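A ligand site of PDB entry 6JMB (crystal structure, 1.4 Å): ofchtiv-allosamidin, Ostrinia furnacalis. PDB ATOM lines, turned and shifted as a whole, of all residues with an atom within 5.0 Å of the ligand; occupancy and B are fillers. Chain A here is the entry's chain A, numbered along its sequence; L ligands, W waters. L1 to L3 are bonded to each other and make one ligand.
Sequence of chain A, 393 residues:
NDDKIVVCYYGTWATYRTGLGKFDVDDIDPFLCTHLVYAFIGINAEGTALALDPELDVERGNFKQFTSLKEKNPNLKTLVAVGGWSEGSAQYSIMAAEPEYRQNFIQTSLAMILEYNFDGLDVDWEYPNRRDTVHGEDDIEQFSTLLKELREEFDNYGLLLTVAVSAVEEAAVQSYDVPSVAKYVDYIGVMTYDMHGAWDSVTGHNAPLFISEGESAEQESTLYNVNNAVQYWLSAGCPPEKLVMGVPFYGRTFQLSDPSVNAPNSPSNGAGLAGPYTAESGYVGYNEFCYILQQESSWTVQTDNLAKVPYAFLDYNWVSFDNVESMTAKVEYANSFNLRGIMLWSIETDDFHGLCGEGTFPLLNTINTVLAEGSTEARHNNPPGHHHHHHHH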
ATOM      1  N   TYR A   9     -15.809  -4.785  23.767  1.00  0.00           N
ATOM      2  CA  TYR A   9     -14.625  -5.081  22.969  1.00  0.00           C
ATOM      3  C   TYR A   9     -14.805  -4.554  21.550  1.00  0.00           C
ATOM      4  O   TYR A   9     -15.906  -4.636  20.980  1.00  0.00           O
ATOM      5  CB  TYR A   9     -14.378  -6.573  22.904  1.00  0.00           C
ATOM      6  CG  TYR A   9     -13.729  -7.141  24.139  1.00  0.00           C
ATOM      7  CD1 TYR A   9     -14.493  -7.526  25.229  1.00  0.00           C
ATOM      8  CD2 TYR A   9     -12.351  -7.295  24.207  1.00  0.00           C
ATOM      9  CE1 TYR A   9     -13.882  -8.041  26.358  1.00  0.00           C
ATOM     10  CE2 TYR A   9     -11.737  -7.815  25.328  1.00  0.00           C
ATOM     11  CZ  TYR A   9     -12.512  -8.206  26.392  1.00  0.00           C
ATOM     12  OH  TYR A   9     -11.930  -8.743  27.524  1.00  0.00           O
ATOM     13  N   TRP A  13      -9.727  -4.611  13.497  1.00  0.00           N
ATOM     14  CA  TRP A  13      -9.589  -4.908  12.076  1.00  0.00           C
ATOM     15  C   TRP A  13     -10.873  -4.635  11.300  1.00  0.00           C
ATOM     16  O   TRP A  13     -10.852  -4.695  10.061  1.00  0.00           O
ATOM     17  CB  TRP A  13      -9.152  -6.372  11.892  1.00  0.00           C
ATOM     18  CG  TRP A  13     -10.010  -7.339  12.637  1.00  0.00           C
ATOM     19  CD1 TRP A  13     -11.114  -7.977  12.167  1.00  0.00           C
ATOM     20  CD2 TRP A  13      -9.849  -7.777  13.997  1.00  0.00           C
ATOM     21  NE1 TRP A  13     -11.655  -8.779  13.149  1.00  0.00           N
ATOM     22  CE2 TRP A  13     -10.895  -8.663  14.283  1.00  0.00           C
ATOM     23  CE3 TRP A  13      -8.918  -7.487  15.003  1.00  0.00           C
ATOM     24  CZ2 TRP A  13     -11.033  -9.283  15.521  1.00  0.00           C
ATOM     25  CZ3 TRP A  13      -9.064  -8.091  16.241  1.00  0.00           C
ATOM     26  CH2 TRP A  13     -10.114  -8.979  16.490  1.00  0.00           C
ATOM     27  N   PHE A  40      -6.553  -6.330  19.013  1.00  0.00           N
ATOM     28  CA  PHE A  40      -5.704  -6.922  20.043  1.00  0.00           C
ATOM     29  C   PHE A  40      -4.276  -6.443  19.834  1.00  0.00           C
ATOM     30  O   PHE A  40      -3.879  -6.145  18.688  1.00  0.00           O
ATOM     31  CB  PHE A  40      -5.639  -8.443  19.893  1.00  0.00           C
ATOM     32  CG  PHE A  40      -6.867  -9.178  20.340  1.00  0.00           C
ATOM     33  CD1 PHE A  40      -7.174  -9.268  21.675  1.00  0.00           C
ATOM     34  CD2 PHE A  40      -7.689  -9.809  19.419  1.00  0.00           C
ATOM     35  CE1 PHE A  40      -8.292  -9.951  22.107  1.00  0.00           C
ATOM     36  CE2 PHE A  40      -8.821 -10.494  19.834  1.00  0.00           C
ATOM     37  CZ  PHE A  40      -9.119 -10.572  21.178  1.00  0.00           C
ATOM     38  N   GLY A  83      -3.557 -10.758  23.307  1.00  0.00           N
ATOM     39  CA  GLY A  83      -3.884 -12.145  23.068  1.00  0.00           C
ATOM     40  C   GLY A  83      -4.933 -12.327  22.003  1.00  0.00           C
ATOM     41  O   GLY A  83      -4.804 -11.810  20.897  1.00  0.00           O
ATOM     42  N   GLY A  84      -5.982 -13.072  22.338  1.00  0.00           N
ATOM     43  CA  GLY A  84      -7.003 -13.410  21.376  1.00  0.00           C
ATOM     44  C   GLY A  84      -6.767 -14.767  20.750  1.00  0.00           C
ATOM     45  O   GLY A  84      -5.671 -15.329  20.788  1.00  0.00           O
ATOM     46  N   TRP A  85      -7.828 -15.291  20.129  1.00  0.00           N
ATOM     47  CA  TRP A  85      -7.775 -16.620  19.517  1.00  0.00           C
ATOM     48  C   TRP A  85      -6.614 -16.764  18.535  1.00  0.00           C
ATOM     49  O   TRP A  85      -5.849 -17.733  18.600  1.00  0.00           O
ATOM     50  CB  TRP A  85      -9.115 -16.892  18.815  1.00  0.00           C
ATOM     51  CG  TRP A  85      -9.166 -18.196  18.102  1.00  0.00           C
ATOM     52  CD1 TRP A  85      -9.084 -18.393  16.748  1.00  0.00           C
ATOM     53  CD2 TRP A  85      -9.318 -19.491  18.677  1.00  0.00           C
ATOM     54  NE1 TRP A  85      -9.178 -19.730  16.453  1.00  0.00           N
ATOM     55  CE2 TRP A  85      -9.322 -20.424  17.623  1.00  0.00           C
ATOM     56  CE3 TRP A  85      -9.459 -19.943  19.996  1.00  0.00           C
ATOM     57  CZ2 TRP A  85      -9.455 -21.797  17.849  1.00  0.00           C
ATOM     58  CZ3 TRP A  85      -9.583 -21.305  20.207  1.00  0.00           C
ATOM     59  CH2 TRP A  85      -9.591 -22.214  19.150  1.00  0.00           C
ATOM     60  N   SER A  86      -6.455 -15.803  17.637  1.00  0.00           N
ATOM     61  CA  SER A  86      -5.430 -15.939  16.589  1.00  0.00           C
ATOM     62  C   SER A  86      -4.017 -15.870  17.145  1.00  0.00           C
ATOM     63  O   SER A  86      -3.076 -16.293  16.458  1.00  0.00           O
ATOM     64  CB  SER A  86      -5.614 -14.870  15.514  1.00  0.00           C
ATOM     65  OG  SER A  86      -6.893 -14.947  14.913  1.00  0.00           O
ATOM     66  N   GLU A  87      -3.818 -15.325  18.343  1.00  0.00           N
ATOM     67  CA  GLU A  87      -2.492 -15.216  18.930  1.00  0.00           C
ATOM     68  C   GLU A  87      -1.993 -16.535  19.512  1.00  0.00           C
ATOM     69  O   GLU A  87      -0.792 -16.660  19.790  1.00  0.00           O
ATOM     70  CB  GLU A  87      -2.485 -14.138  20.020  1.00  0.00           C
ATOM     71  CG  GLU A  87      -2.037 -12.762  19.528  1.00  0.00           C
ATOM     72  CD  GLU A  87      -0.536 -12.688  19.405  1.00  0.00           C
ATOM     73  OE1 GLU A  87       0.166 -12.667  20.453  1.00  0.00           O
ATOM     74  OE2 GLU A  87      -0.049 -12.655  18.255  1.00  0.00           O
ATOM     75  N   ASP A 122      -6.146  -5.817  29.478  1.00  0.00           N
ATOM     76  CA  ASP A 122      -6.977  -7.012  29.516  1.00  0.00           C
ATOM     77  C   ASP A 122      -6.154  -8.155  28.949  1.00  0.00           C
ATOM     78  O   ASP A 122      -5.584  -8.027  27.858  1.00  0.00           O
ATOM     79  CB  ASP A 122      -8.234  -6.803  28.678  1.00  0.00           C
ATOM     80  CG  ASP A 122      -9.147  -8.008  28.691  1.00  0.00           C
ATOM     81  OD1 ASP A 122      -9.486  -8.505  29.794  1.00  0.00           O
ATOM     82  OD2 ASP A 122      -9.548  -8.465  27.598  1.00  0.00           O
ATOM     83  N   ASP A 124      -6.075 -11.823  27.441  1.00  0.00           N
ATOM     84  CA  ASP A 124      -6.891 -12.811  26.761  1.00  0.00           C
ATOM     85  C   ASP A 124      -5.996 -13.903  26.166  1.00  0.00           C
ATOM     86  O   ASP A 124      -5.946 -14.097  24.945  1.00  0.00           O
ATOM     87  CB  ASP A 124      -7.717 -12.115  25.665  1.00  0.00           C
ATOM     88  CG  ASP A 124      -8.612 -13.065  24.885  1.00  0.00           C
ATOM     89  OD1 ASP A 124      -8.988 -14.124  25.420  1.00  0.00           O
ATOM     90  OD2 ASP A 124      -8.944 -12.730  23.733  1.00  0.00           O
ATOM     91  N   GLU A 126      -5.393 -17.424  25.114  1.00  0.00           N
ATOM     92  CA  GLU A 126      -6.279 -18.522  24.731  1.00  0.00           C
ATOM     93  C   GLU A 126      -5.455 -19.744  24.334  1.00  0.00           C
ATOM     94  O   GLU A 126      -5.113 -19.903  23.161  1.00  0.00           O
ATOM     95  CB  GLU A 126      -7.250 -18.052  23.620  1.00  0.00           C
ATOM     96  CG  GLU A 126      -8.038 -16.811  24.043  1.00  0.00           C
ATOM     97  CD  GLU A 126      -9.305 -16.555  23.247  1.00  0.00           C
ATOM     98  OE1 GLU A 126      -9.569 -17.254  22.251  1.00  0.00           O
ATOM     99  OE2 GLU A 126     -10.047 -15.629  23.643  1.00  0.00           O
ATOM    100  N   ALA A 164     -10.021 -12.068  30.212  1.00  0.00           N
ATOM    101  CA  ALA A 164     -11.103 -12.759  29.537  1.00  0.00           C
ATOM    102  C   ALA A 164     -10.795 -14.246  29.625  1.00  0.00           C
ATOM    103  O   ALA A 164      -9.651 -14.657  29.383  1.00  0.00           O
ATOM    104  CB  ALA A 164     -11.181 -12.360  28.061  1.00  0.00           C
ATOM    105  N   MET A 191     -16.259 -15.600  28.969  1.00  0.00           N
ATOM    106  CA  MET A 191     -16.656 -15.636  27.552  1.00  0.00           C
ATOM    107  C   MET A 191     -17.764 -16.661  27.350  1.00  0.00           C
ATOM    108  O   MET A 191     -17.577 -17.746  26.786  1.00  0.00           O
ATOM    109  CB  MET A 191     -15.438 -15.913  26.670  1.00  0.00           C
ATOM    110  CG  MET A 191     -14.433 -14.777  26.670  1.00  0.00           C
ATOM    111  SD  MET A 191     -13.114 -14.987  25.455  1.00  0.00           S
ATOM    112  CE  MET A 191     -12.103 -16.210  26.287  1.00  0.00           C
ATOM    113  N   TYR A 193     -20.058 -17.618  25.419  1.00  0.00           N
ATOM    114  CA  TYR A 193     -20.493 -17.784  24.042  1.00  0.00           C
ATOM    115  C   TYR A 193     -19.513 -18.761  23.395  1.00  0.00           C
ATOM    116  O   TYR A 193     -18.637 -19.311  24.067  1.00  0.00           O
ATOM    117  CB  TYR A 193     -20.597 -16.441  23.295  1.00  0.00           C
ATOM    118  CG  TYR A 193     -19.519 -15.451  23.654  1.00  0.00           C
ATOM    119  CD1 TYR A 193     -18.207 -15.630  23.224  1.00  0.00           C
ATOM    120  CD2 TYR A 193     -19.800 -14.326  24.429  1.00  0.00           C
ATOM    121  CE1 TYR A 193     -17.211 -14.722  23.554  1.00  0.00           C
ATOM    122  CE2 TYR A 193     -18.814 -13.417  24.754  1.00  0.00           C
ATOM    123  CZ  TYR A 193     -17.528 -13.622  24.318  1.00  0.00           C
ATOM    124  OH  TYR A 193     -16.545 -12.721  24.646  1.00  0.00           O
ATOM    125  N   ASP A 194     -19.668 -18.996  22.088  1.00  0.00           N
ATOM    126  CA  ASP A 194     -18.939 -20.071  21.422  1.00  0.00           C
ATOM    127  C   ASP A 194     -19.204 -21.417  22.085  1.00  0.00           C
ATOM    128  O   ASP A 194     -18.358 -22.318  22.065  1.00  0.00           O
ATOM    129  CB  ASP A 194     -17.438 -19.801  21.316  1.00  0.00           C
ATOM    130  CG  ASP A 194     -17.141 -18.471  20.674  1.00  0.00           C
ATOM    131  OD1 ASP A 194     -17.814 -18.126  19.686  1.00  0.00           O
ATOM    132  OD2 ASP A 194     -16.220 -17.772  21.151  1.00  0.00           O
ATOM    133  N   TYR A 250     -22.645 -11.620  17.523  1.00  0.00           N
ATOM    134  CA  TYR A 250     -22.517 -12.360  16.291  1.00  0.00           C
ATOM    135  C   TYR A 250     -23.213 -13.694  16.497  1.00  0.00           C
ATOM    136  O   TYR A 250     -23.505 -14.101  17.637  1.00  0.00           O
ATOM    137  CB  TYR A 250     -21.031 -12.605  15.939  1.00  0.00           C
ATOM    138  CG  TYR A 250     -20.329 -13.411  17.007  1.00  0.00           C
ATOM    139  CD1 TYR A 250     -19.843 -12.800  18.160  1.00  0.00           C
ATOM    140  CD2 TYR A 250     -20.163 -14.789  16.880  1.00  0.00           C
ATOM    141  CE1 TYR A 250     -19.233 -13.529  19.149  1.00  0.00           C
ATOM    142  CE2 TYR A 250     -19.548 -15.529  17.877  1.00  0.00           C
ATOM    143  CZ  TYR A 250     -19.084 -14.890  19.018  1.00  0.00           C
ATOM    144  OH  TYR A 250     -18.464 -15.608  20.015  1.00  0.00           O
ATOM    145  N   ARG A 252     -23.469 -17.952  14.758  1.00  0.00           N
ATOM    146  CA  ARG A 252     -22.691 -19.001  14.118  1.00  0.00           C
ATOM    147  C   ARG A 252     -23.574 -19.787  13.159  1.00  0.00           C
ATOM    148  O   ARG A 252     -24.776 -19.953  13.396  1.00  0.00           O
ATOM    149  CB  ARG A 252     -21.991 -19.892  15.151  1.00  0.00           C
ATOM    150  CG  ARG A 252     -20.945 -19.110  15.941  1.00  0.00           C
ATOM    151  CD  ARG A 252     -20.023 -20.008  16.753  1.00  0.00           C
ATOM    152  NE  ARG A 252     -18.874 -19.243  17.236  1.00  0.00           N
ATOM    153  CZ  ARG A 252     -17.813 -18.926  16.502  1.00  0.00           C
ATOM    154  NH1 ARG A 252     -17.742 -19.324  15.240  1.00  0.00           N
ATOM    155  NH2 ARG A 252     -16.819 -18.203  17.027  1.00  0.00           N
ATOM    156  N   THR A 278     -17.938  -9.610   7.155  1.00  0.00           N
ATOM    157  CA  THR A 278     -17.047 -10.433   7.972  1.00  0.00           C
ATOM    158  C   THR A 278     -16.399 -11.535   7.134  1.00  0.00           C
ATOM    159  O   THR A 278     -15.265 -11.929   7.403  1.00  0.00           O
ATOM    160  CB  THR A 278     -17.793 -10.986   9.181  1.00  0.00           C
ATOM    161  OG1 THR A 278     -19.005 -11.621   8.744  1.00  0.00           O
ATOM    162  CG2 THR A 278     -18.157  -9.860  10.144  1.00  0.00           C
ATOM    163  N   GLU A 280     -16.447 -14.845   6.525  1.00  0.00           N
ATOM    164  CA  GLU A 280     -15.887 -16.093   7.038  1.00  0.00           C
ATOM    165  C   GLU A 280     -17.015 -17.086   7.236  1.00  0.00           C
ATOM    166  O   GLU A 280     -17.875 -16.882   8.097  1.00  0.00           O
ATOM    167  CB  GLU A 280     -15.142 -15.856   8.350  1.00  0.00           C
ATOM    168  CG  GLU A 280     -14.311 -17.034   8.809  1.00  0.00           C
ATOM    169  CD  GLU A 280     -13.225 -17.399   7.810  1.00  0.00           C
ATOM    170  OE1 GLU A 280     -12.531 -16.480   7.327  1.00  0.00           O
ATOM    171  OE2 GLU A 280     -13.065 -18.596   7.499  1.00  0.00           O
ATOM    172  N   TYR A 283     -19.620 -17.951  10.719  1.00  0.00           N
ATOM    173  CA  TYR A 283     -20.121 -16.942  11.654  1.00  0.00           C
ATOM    174  C   TYR A 283     -20.645 -15.752  10.859  1.00  0.00           C
ATOM    175  O   TYR A 283     -20.359 -15.589   9.668  1.00  0.00           O
ATOM    176  CB  TYR A 283     -19.095 -16.564  12.739  1.00  0.00           C
ATOM    177  CG  TYR A 283     -18.178 -15.399  12.422  1.00  0.00           C
ATOM    178  CD1 TYR A 283     -16.974 -15.608  11.762  1.00  0.00           C
ATOM    179  CD2 TYR A 283     -18.489 -14.106  12.828  1.00  0.00           C
ATOM    180  CE1 TYR A 283     -16.123 -14.550  11.485  1.00  0.00           C
ATOM    181  CE2 TYR A 283     -17.638 -13.048  12.551  1.00  0.00           C
ATOM    182  CZ  TYR A 283     -16.456 -13.274  11.881  1.00  0.00           C
ATOM    183  OH  TYR A 283     -15.606 -12.230  11.600  1.00  0.00           O
ATOM    184  N   MET A 343     -20.247  -8.097  29.408  1.00  0.00           N
ATOM    185  CA  MET A 343     -19.150  -7.936  28.464  1.00  0.00           C
ATOM    186  C   MET A 343     -19.682  -8.362  27.097  1.00  0.00           C
ATOM    187  O   MET A 343     -20.502  -9.290  27.002  1.00  0.00           O
ATOM    188  CB  MET A 343     -17.989  -8.857  28.875  1.00  0.00           C
ATOM    189  CG  MET A 343     -16.827  -8.910  27.912  1.00  0.00           C
ATOM    190  SD  MET A 343     -15.512 -10.018  28.480  1.00  0.00           S
ATOM    191  CE  MET A 343     -16.169 -11.628  28.071  1.00  0.00           C
ATOM    192  N   TRP A 345     -18.641  -9.272  22.940  1.00  0.00           N
ATOM    193  CA  TRP A 345     -17.817  -9.421  21.741  1.00  0.00           C
ATOM    194  C   TRP A 345     -18.782  -9.416  20.569  1.00  0.00           C
ATOM    195  O   TRP A 345     -19.554 -10.370  20.410  1.00  0.00           O
ATOM    196  CB  TRP A 345     -17.041 -10.742  21.764  1.00  0.00           C
ATOM    197  CG  TRP A 345     -16.132 -10.781  20.579  1.00  0.00           C
ATOM    198  CD1 TRP A 345     -16.436 -11.225  19.318  1.00  0.00           C
ATOM    199  CD2 TRP A 345     -14.801 -10.250  20.523  1.00  0.00           C
ATOM    200  NE1 TRP A 345     -15.353 -11.033  18.485  1.00  0.00           N
ATOM    201  CE2 TRP A 345     -14.344 -10.433  19.199  1.00  0.00           C
ATOM    202  CE3 TRP A 345     -13.949  -9.662  21.456  1.00  0.00           C
ATOM    203  CZ2 TRP A 345     -13.062 -10.036  18.790  1.00  0.00           C
ATOM    204  CZ3 TRP A 345     -12.692  -9.264  21.051  1.00  0.00           C
ATOM    205  CH2 TRP A 345     -12.260  -9.460  19.725  1.00  0.00           C
HETATM  206  C1  LIG L   1      -9.965 -12.674  12.606  1.00  0.00           C
HETATM  207  C2  LIG L   1      -8.713 -12.264  11.849  1.00  0.00           C
HETATM  208  C3  LIG L   1      -9.023 -11.824  10.447  1.00  0.00           C
HETATM  209  C4  LIG L   1      -9.814 -12.838   9.681  1.00  0.00           C
HETATM  210  C5  LIG L   1     -11.061 -13.246  10.475  1.00  0.00           C
HETATM  211  C6  LIG L   1     -11.769 -14.405   9.888  1.00  0.00           C
HETATM  212  C7  LIG L   1      -6.962 -11.309  13.499  1.00  0.00           C
HETATM  213  C8  LIG L   1      -6.372 -10.094  14.254  1.00  0.00           C
HETATM  214  N1  LIG L   1      -8.123 -11.107  12.578  1.00  0.00           N
HETATM  215  O1  LIG L   1      -9.887 -10.667  10.551  1.00  0.00           O
HETATM  216  O2  LIG L   1     -10.257 -12.208   8.471  1.00  0.00           O
HETATM  217  O3  LIG L   1     -10.703 -13.712  11.837  1.00  0.00           O
HETATM  218  O4  LIG L   1     -12.443 -15.024  10.992  1.00  0.00           O
HETATM  219  O5  LIG L   1      -6.488 -12.417  13.652  1.00  0.00           O
HETATM  220  C1  LG2 L   2     -12.145 -13.780  17.119  1.00  0.00           C
HETATM  221  C2  LG2 L   2     -12.778 -13.373  15.803  1.00  0.00           C
HETATM  222  C3  LG2 L   2     -11.897 -13.635  14.643  1.00  0.00           C
HETATM  223  C4  LG2 L   2     -10.558 -12.944  14.825  1.00  0.00           C
HETATM  224  C5  LG2 L   2      -9.934 -13.395  16.140  1.00  0.00           C
HETATM  225  C6  LG2 L   2      -8.621 -12.726  16.434  1.00  0.00           C
HETATM  226  C7  LG2 L   2     -15.335 -13.475  15.816  1.00  0.00           C
HETATM  227  C8  LG2 L   2     -16.615 -14.325  15.788  1.00  0.00           C
HETATM  228  N1  LG2 L   2     -14.045 -14.183  15.744  1.00  0.00           N
HETATM  229  O1  LG2 L   2     -11.730 -15.078  14.531  1.00  0.00           O
HETATM  230  O2  LG2 L   2      -9.627 -13.266  13.768  1.00  0.00           O
HETATM  231  O3  LG2 L   2     -10.844 -13.056  17.230  1.00  0.00           O
HETATM  232  O4  LG2 L   2      -8.122 -13.293  17.627  1.00  0.00           O
HETATM  233  O5  LG2 L   2     -15.374 -12.304  15.869  1.00  0.00           O
HETATM  234  C1  LG3 L   3     -13.343 -14.126  21.692  1.00  0.00           C
HETATM  235  C2  LG3 L   3     -11.763 -13.979  21.603  1.00  0.00           C
HETATM  236  C3  LG3 L   3     -11.546 -13.441  20.284  1.00  0.00           C
HETATM  237  C4  LG3 L   3     -12.709 -14.035  19.401  1.00  0.00           C
HETATM  238  C5  LG3 L   3     -13.859 -13.794  20.268  1.00  0.00           C
HETATM  239  C6  LG3 L   3     -15.121 -14.645  19.881  1.00  0.00           C
HETATM  240  C7  LG3 L   3     -12.596 -12.619  23.135  1.00  0.00           C
HETATM  241  C8  LG3 L   3     -11.358 -11.143  24.812  1.00  0.00           C
HETATM  242  C9  LG3 L   3     -13.925 -11.160  24.770  1.00  0.00           C
HETATM  243  N1  LG3 L   3     -11.431 -13.160  22.564  1.00  0.00           N
HETATM  244  N2  LG3 L   3     -12.618 -11.641  24.238  1.00  0.00           N
HETATM  245  O1  LG3 L   3     -10.241 -13.786  19.817  1.00  0.00           O
HETATM  246  O2  LG3 L   3     -12.951 -13.360  18.175  1.00  0.00           O
HETATM  247  O3  LG3 L   3     -14.751 -16.008  19.832  1.00  0.00           O
HETATM  248  O4  LG3 L   3     -13.756 -13.084  22.603  1.00  0.00           O
HETATM  249  O   HOH W   1      -8.652  -8.410   8.777  1.00  0.00           O
HETATM  250  O   HOH W   2     -14.001 -16.845  17.235  1.00  0.00           O
HETATM  251  O   HOH W   3     -13.913 -10.752  13.416  1.00  0.00           O
HETATM  252  O   HOH W   4     -17.396 -10.625  14.872  1.00  0.00           O
HETATM  253  O   HOH W   5     -12.121 -17.510  21.198  1.00  0.00           O
HETATM  254  O   HOH W   6     -13.944 -12.217   9.520  1.00  0.00           O
HETATM  255  O   HOH W   7      -5.652 -12.407  18.370  1.00  0.00           O
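The side-chain carboxylate (OD2) of Asp 194 sits at hydrogen-bond distance from an oxygen (O3) of LG3 L3, at 2.6 Å. The side-chain carboxylate (OD2) of Asp 124 sits at hydrogen-bond distance from a nitrogen (N1) of LG3 L3 (2.8 Å). O4 of LG2 L2 lies within hydrogen-bond range of N of Ser 86 (3.0 Å). The side-chain hydroxyl of Ser 86 is in hydrogen-bond range of an oxygen (O5) of LIG L1 (2.9 Å). The backbone NH of Trp 85 is in hydrogen-bond range of an oxygen (O1) of LG3 L3, 2.9 Å away. The indole nitrogen (NE1) of Trp 345 is in hydrogen-bond range of an oxygen (O5) of LG2 L2. The side-chain hydroxyl (OH) of Tyr 193 sits close to an oxygen (O4) of LG3 L3 (3.5 Å).
OE2 of Glu 126 sits close to N1 of LG3 L3 (3.0 Å). The side-chain sulfur (SD) of Met 191 lies close to an oxygen (O4) of LG3 L3. Merely in contact with the ligand: Tyr 9, Trp 13, Phe 40, Gly 84, Ala 164, Tyr 250, Glu 280 and Tyr 283. Hydrophobic or aromatic side chains that line the ligand: Tyr 9, Trp 13, Phe 40, Trp 85, Ala 164, Met 191, Tyr 193, Tyr 250, Tyr 283 and Trp 345. Within 4 Å of the ligand: Tyr 9, Trp 13, Phe 40, Gly 84, Trp 85, Ser 86, Asp 124, Glu 126, Ala 164, Met 191, Tyr 193, Asp 194, Tyr 250, Glu 280, Tyr 283 and Trp 345. The nearest printed residue that does not touch the ligand is Met 343 (4.02 Å).
OH of Tyr 250 sits at hydrogen-bond distance from OD1 of Asp 194. OD1 of Asp 194 lies within salt-bridge range of NH2 of Arg 252, at 2.8 Å. The side-chain carboxylate of Asp 124 lies close to the side-chain carboxylate of Glu 126 (2.6 Å). O of Asp 124 lies within hydrogen-bond range of N of Gly 84. OE1 of Glu 126 lies close to N of Trp 85 (3.4 Å). The side-chain carboxylate (OD1) of Asp 122 lies close to the side-chain hydroxyl (OH) of Tyr 9 (3.3 Å).
Water W7 lies within hydrogen-bond range of an oxygen (O4) of LG2 L2, the backbone carbonyl oxygen (O) of Gly 83 and the backbone NH (N) of Glu 87. Water W2 bridges an oxygen (O3) of LG3 L3 and the guanidinium group (NH2) of Arg 252. Water W6 lies within hydrogen-bond range of the backbone carbonyl oxygen of Thr 278 (2.5 Å) and the side-chain hydroxyl of Tyr 283 (2.7 Å). Water W3 lies within hydrogen-bond range of the side-chain hydroxyl (OH) of Tyr 283 (2.9 Å), the indole nitrogen (NE1) of Trp 13 (3.0 Å) and an oxygen (O5) of LG2 L2 (3.2 Å). Water W5 bridges OE1 of Glu 126 (2.8 Å) and O3 of LG3 L3 (3.3 Å).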
